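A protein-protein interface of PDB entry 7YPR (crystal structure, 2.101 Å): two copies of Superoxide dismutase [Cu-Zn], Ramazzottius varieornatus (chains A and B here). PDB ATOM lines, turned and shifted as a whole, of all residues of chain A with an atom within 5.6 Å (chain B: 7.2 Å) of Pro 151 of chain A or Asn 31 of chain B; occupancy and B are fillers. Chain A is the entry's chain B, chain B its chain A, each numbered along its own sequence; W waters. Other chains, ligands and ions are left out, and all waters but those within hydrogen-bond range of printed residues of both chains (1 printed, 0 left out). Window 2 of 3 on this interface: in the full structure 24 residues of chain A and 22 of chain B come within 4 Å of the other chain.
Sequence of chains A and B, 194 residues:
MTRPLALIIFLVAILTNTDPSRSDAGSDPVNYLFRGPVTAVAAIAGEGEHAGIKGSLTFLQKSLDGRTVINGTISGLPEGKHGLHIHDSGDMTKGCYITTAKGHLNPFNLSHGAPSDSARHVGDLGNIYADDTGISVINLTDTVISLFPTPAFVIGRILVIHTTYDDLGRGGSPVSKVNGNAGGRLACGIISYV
CB of Pro 107 of chain A touches CE1 of Tyr 32 of chain B, at 3.998 Å.
O of Pro 149 of chain A touches CD1 of Leu 33 of chain B, 3.7 Å away.
CB of Pro 149 of chain A touches CB of Pro 149 of chain B (3.5 Å).
Thr 150 of chain A touches Asn 31 of chain B (CA to ND2, 3.5 Å).
Leu 33 of chain B touches Thr 150 of chain A.
Asn 31 of chain B touches Pro 151 of chain A (ND2 to N, 3.8 Å).
Tyr 32 of chain B touches Pro 151 of chain A.
Leu 33 of chain B touches Phe 153 of chain A.
Pro 151 of chain A touches two residues of chain B.
Of the printed residues of chain A, Asn 31 of chain B touches Pro 149, Thr 150 and Pro 151.
Printed residues of chain B within 4 Å of Phe 153 of chain A: Leu 33 (3.5 Å).
Printed residues of chain B within 4 Å of Thr 150 of chain A: Asn 31 and Leu 33.
The nearest printed residue of chain A that does not touch Asn 31 of chain B is Ala 152 of chain A (6.4 Å).
The nearest printed residue of chain B that does not touch Pro 107 of chain A is Leu 33 of chain B (7.7 Å).
Of the 8 printed residues of chain A, 5 touch a printed residue of chain B.
Of the 7 printed residues of chain B, 4 touch a printed residue of chain A.
Among the printed residues, 9 pairs touch across the chains.
Among the printed residues, no Asp or Glu carboxylate lies within 4 Å of a Lys or Arg side-chain nitrogen of the other chain.
Pro 149 of chain A touches its own counterpart, Pro 149 of chain B.
1 position is printed for both chains.
Of the 9 pairs that touch across the chains among the printed residues, 1 has its exchanged pair printed and touching as well.
The backbone carbonyl oxygen of Pro 149 of chain A sits at hydrogen-bond distance from the side-chain amide nitrogen of Asn 31 of chain B, 2.8 Å away.
The side-chain amide oxygen of Asn 31 of chain B lies within hydrogen-bond range of the backbone NH of Leu 33 of chain B.
N of Ala 152 of chain A sits close to OG1 of Thr 150 of chain A, at 3.3 Å.
Water W1 lies within hydrogen-bond range of OH of Tyr 32 of chain B, O of Phe 153 of chain A and O of Pro 151 of chain A.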
ATOM      1  N   PRO A 107      20.888 -24.714 -16.174  1.00  0.00           N
ATOM      2  CA  PRO A 107      21.468 -25.203 -14.915  1.00  0.00           C
ATOM      3  C   PRO A 107      21.407 -24.204 -13.765  1.00  0.00           C
ATOM      4  O   PRO A 107      21.634 -24.602 -12.620  1.00  0.00           O
ATOM      5  CB  PRO A 107      22.927 -25.493 -15.298  1.00  0.00           C
ATOM      6  CG  PRO A 107      23.194 -24.505 -16.402  1.00  0.00           C
ATOM      7  CD  PRO A 107      21.929 -24.509 -17.203  1.00  0.00           C
ATOM      8  N   PHE A 108      21.160 -22.923 -14.026  1.00  0.00           N
ATOM      9  CA  PHE A 108      21.128 -21.911 -12.974  1.00  0.00           C
ATOM     10  C   PHE A 108      19.706 -21.522 -12.593  1.00  0.00           C
ATOM     11  O   PHE A 108      19.525 -20.590 -11.803  1.00  0.00           O
ATOM     12  CB  PHE A 108      21.938 -20.676 -13.397  1.00  0.00           C
ATOM     13  CG  PHE A 108      23.342 -21.007 -13.859  1.00  0.00           C
ATOM     14  CD1 PHE A 108      24.159 -21.829 -13.093  1.00  0.00           C
ATOM     15  CD2 PHE A 108      23.824 -20.527 -15.067  1.00  0.00           C
ATOM     16  CE1 PHE A 108      25.453 -22.169 -13.526  1.00  0.00           C
ATOM     17  CE2 PHE A 108      25.126 -20.844 -15.501  1.00  0.00           C
ATOM     18  CZ  PHE A 108      25.933 -21.673 -14.728  1.00  0.00           C
ATOM     19  N   VAL A 122      21.062 -20.442 -19.814  1.00  0.00           N
ATOM     20  CA  VAL A 122      22.317 -20.635 -20.545  1.00  0.00           C
ATOM     21  C   VAL A 122      22.029 -20.799 -22.030  1.00  0.00           C
ATOM     22  O   VAL A 122      22.708 -20.213 -22.879  1.00  0.00           O
ATOM     23  CB  VAL A 122      23.109 -21.838 -19.990  1.00  0.00           C
ATOM     24  CG1 VAL A 122      24.232 -22.231 -20.963  1.00  0.00           C
ATOM     25  CG2 VAL A 122      23.732 -21.489 -18.639  1.00  0.00           C
ATOM     26  N   PRO A 149      33.902 -28.054 -19.426  1.00  0.00           N
ATOM     27  CA  PRO A 149      32.887 -28.755 -18.606  1.00  0.00           C
ATOM     28  C   PRO A 149      32.676 -28.144 -17.226  1.00  0.00           C
ATOM     29  O   PRO A 149      32.792 -28.812 -16.201  1.00  0.00           O
ATOM     30  CB  PRO A 149      33.454 -30.175 -18.520  1.00  0.00           C
ATOM     31  CG  PRO A 149      34.565 -30.238 -19.542  1.00  0.00           C
ATOM     32  CD  PRO A 149      35.112 -28.863 -19.606  1.00  0.00           C
ATOM     33  N   THR A 150      32.336 -26.859 -17.200  1.00  0.00           N
ATOM     34  CA  THR A 150      31.762 -26.182 -16.037  1.00  0.00           C
ATOM     35  C   THR A 150      30.241 -26.347 -16.082  1.00  0.00           C
ATOM     36  O   THR A 150      29.724 -26.891 -17.067  1.00  0.00           O
ATOM     37  CB  THR A 150      32.138 -24.700 -16.072  1.00  0.00           C
ATOM     38  OG1 THR A 150      31.380 -24.085 -17.115  1.00  0.00           O
ATOM     39  CG2 THR A 150      33.640 -24.505 -16.350  1.00  0.00           C
ATOM     40  N   PRO A 151      29.478 -25.877 -15.084  1.00  0.00           N
ATOM     41  CA  PRO A 151      28.012 -26.003 -15.184  1.00  0.00           C
ATOM     42  C   PRO A 151      27.388 -25.340 -16.412  1.00  0.00           C
ATOM     43  O   PRO A 151      26.244 -25.665 -16.735  1.00  0.00           O
ATOM     44  CB  PRO A 151      27.509 -25.351 -13.888  1.00  0.00           C
ATOM     45  CG  PRO A 151      28.663 -25.457 -12.937  1.00  0.00           C
ATOM     46  CD  PRO A 151      29.887 -25.336 -13.768  1.00  0.00           C
ATOM     47  N   ALA A 152      28.077 -24.447 -17.122  1.00  0.00           N
ATOM     48  CA  ALA A 152      27.484 -23.847 -18.312  1.00  0.00           C
ATOM     49  C   ALA A 152      27.846 -24.601 -19.590  1.00  0.00           C
ATOM     50  O   ALA A 152      27.637 -24.073 -20.678  1.00  0.00           O
ATOM     51  CB  ALA A 152      27.900 -22.373 -18.435  1.00  0.00           C
ATOM     52  N   PHE A 153      28.436 -25.789 -19.463  1.00  0.00           N
ATOM     53  CA  PHE A 153      28.813 -26.630 -20.599  1.00  0.00           C
ATOM     54  C   PHE A 153      27.640 -26.815 -21.548  1.00  0.00           C
ATOM     55  O   PHE A 153      26.566 -27.239 -21.117  1.00  0.00           O
ATOM     56  CB  PHE A 153      29.234 -27.986 -20.041  1.00  0.00           C
ATOM     57  CG  PHE A 153      30.086 -28.839 -20.960  1.00  0.00           C
ATOM     58  CD1 PHE A 153      31.126 -28.303 -21.692  1.00  0.00           C
ATOM     59  CD2 PHE A 153      29.889 -30.212 -20.996  1.00  0.00           C
ATOM     60  CE1 PHE A 153      31.941 -29.114 -22.469  1.00  0.00           C
ATOM     61  CE2 PHE A 153      30.700 -31.025 -21.780  1.00  0.00           C
ATOM     62  CZ  PHE A 153      31.724 -30.480 -22.501  1.00  0.00           C
ATOM     63  N   VAL B  30      28.648 -30.006  -5.902  1.00  0.00           N
ATOM     64  CA  VAL B  30      29.679 -30.054  -6.930  1.00  0.00           C
ATOM     65  C   VAL B  30      29.020 -29.823  -8.291  1.00  0.00           C
ATOM     66  O   VAL B  30      27.804 -29.986  -8.425  1.00  0.00           O
ATOM     67  CB  VAL B  30      30.468 -31.402  -6.895  1.00  0.00           C
ATOM     68  CG1 VAL B  30      31.344 -31.488  -5.651  1.00  0.00           C
ATOM     69  CG2 VAL B  30      29.527 -32.598  -6.960  1.00  0.00           C
ATOM     70  N   ASN B  31      29.822 -29.417  -9.276  1.00  0.00           N
ATOM     71  CA  ASN B  31      29.418 -29.307 -10.677  1.00  0.00           C
ATOM     72  C   ASN B  31      28.587 -30.514 -11.105  1.00  0.00           C
ATOM     73  O   ASN B  31      29.061 -31.649 -11.067  1.00  0.00           O
ATOM     74  CB  ASN B  31      30.689 -29.173 -11.527  1.00  0.00           C
ATOM     75  CG  ASN B  31      30.440 -29.181 -13.045  1.00  0.00           C
ATOM     76  OD1 ASN B  31      29.377 -29.537 -13.535  1.00  0.00           O
ATOM     77  ND2 ASN B  31      31.465 -28.812 -13.787  1.00  0.00           N
ATOM     78  N   TYR B  32      27.335 -30.266 -11.510  1.00  0.00           N
ATOM     79  CA  TYR B  32      26.386 -31.349 -11.763  1.00  0.00           C
ATOM     80  C   TYR B  32      26.816 -32.278 -12.894  1.00  0.00           C
ATOM     81  O   TYR B  32      26.285 -33.388 -12.999  1.00  0.00           O
ATOM     82  CB  TYR B  32      25.009 -30.779 -12.082  1.00  0.00           C
ATOM     83  CG  TYR B  32      24.805 -30.372 -13.527  1.00  0.00           C
ATOM     84  CD1 TYR B  32      25.365 -29.196 -14.021  1.00  0.00           C
ATOM     85  CD2 TYR B  32      24.029 -31.148 -14.392  1.00  0.00           C
ATOM     86  CE1 TYR B  32      25.171 -28.802 -15.337  1.00  0.00           C
ATOM     87  CE2 TYR B  32      23.819 -30.760 -15.721  1.00  0.00           C
ATOM     88  CZ  TYR B  32      24.401 -29.582 -16.182  1.00  0.00           C
ATOM     89  OH  TYR B  32      24.226 -29.173 -17.486  1.00  0.00           O
ATOM     90  N   LEU B  33      27.741 -31.852 -13.752  1.00  0.00           N
ATOM     91  CA  LEU B  33      28.239 -32.754 -14.783  1.00  0.00           C
ATOM     92  C   LEU B  33      29.017 -33.912 -14.188  1.00  0.00           C
ATOM     93  O   LEU B  33      29.217 -34.927 -14.868  1.00  0.00           O
ATOM     94  CB  LEU B  33      29.133 -31.995 -15.764  1.00  0.00           C
ATOM     95  CG  LEU B  33      28.501 -30.863 -16.587  1.00  0.00           C
ATOM     96  CD1 LEU B  33      29.590 -30.200 -17.390  1.00  0.00           C
ATOM     97  CD2 LEU B  33      27.415 -31.372 -17.533  1.00  0.00           C
ATOM     98  N   PHE B  34      29.470 -33.773 -12.940  1.00  0.00           N
ATOM     99  CA  PHE B  34      30.273 -34.779 -12.266  1.00  0.00           C
ATOM    100  C   PHE B  34      29.474 -35.600 -11.257  1.00  0.00           C
ATOM    101  O   PHE B  34      30.071 -36.350 -10.482  1.00  0.00           O
ATOM    102  CB  PHE B  34      31.467 -34.116 -11.570  1.00  0.00           C
ATOM    103  CG  PHE B  34      32.569 -33.710 -12.515  1.00  0.00           C
ATOM    104  CD1 PHE B  34      32.529 -32.482 -13.162  1.00  0.00           C
ATOM    105  CD2 PHE B  34      33.631 -34.562 -12.772  1.00  0.00           C
ATOM    106  CE1 PHE B  34      33.541 -32.103 -14.029  1.00  0.00           C
ATOM    107  CE2 PHE B  34      34.639 -34.203 -13.643  1.00  0.00           C
ATOM    108  CZ  PHE B  34      34.600 -32.969 -14.274  1.00  0.00           C
ATOM    109  N   ARG B  35      28.147 -35.512 -11.279  1.00  0.00           N
ATOM    110  CA  ARG B  35      27.296 -36.071 -10.236  1.00  0.00           C
ATOM    111  C   ARG B  35      26.418 -37.203 -10.760  1.00  0.00           C
ATOM    112  O   ARG B  35      26.021 -37.211 -11.929  1.00  0.00           O
ATOM    113  CB  ARG B  35      26.394 -34.970  -9.642  1.00  0.00           C
ATOM    114  CG  ARG B  35      25.419 -35.437  -8.542  1.00  0.00           C
ATOM    115  CD  ARG B  35      25.071 -34.331  -7.527  1.00  0.00           C
ATOM    116  NE  ARG B  35      24.687 -33.066  -8.150  1.00  0.00           N
ATOM    117  CZ  ARG B  35      25.336 -31.919  -7.991  1.00  0.00           C
ATOM    118  NH1 ARG B  35      26.442 -31.846  -7.267  1.00  0.00           N
ATOM    119  NH2 ARG B  35      24.865 -30.817  -8.575  1.00  0.00           N
ATOM    120  N   PRO B 149      33.322 -35.696 -17.199  1.00  0.00           N
ATOM    121  CA  PRO B 149      34.396 -34.951 -17.876  1.00  0.00           C
ATOM    122  C   PRO B 149      35.801 -35.216 -17.345  1.00  0.00           C
ATOM    123  O   PRO B 149      36.548 -34.273 -17.074  1.00  0.00           O
ATOM    124  CB  PRO B 149      33.989 -33.490 -17.655  1.00  0.00           C
ATOM    125  CG  PRO B 149      32.483 -33.558 -17.460  1.00  0.00           C
ATOM    126  CD  PRO B 149      32.360 -34.777 -16.570  1.00  0.00           C
HETATM  127  O   HOH W   1      25.328 -27.187 -18.742  1.00  0.00           O
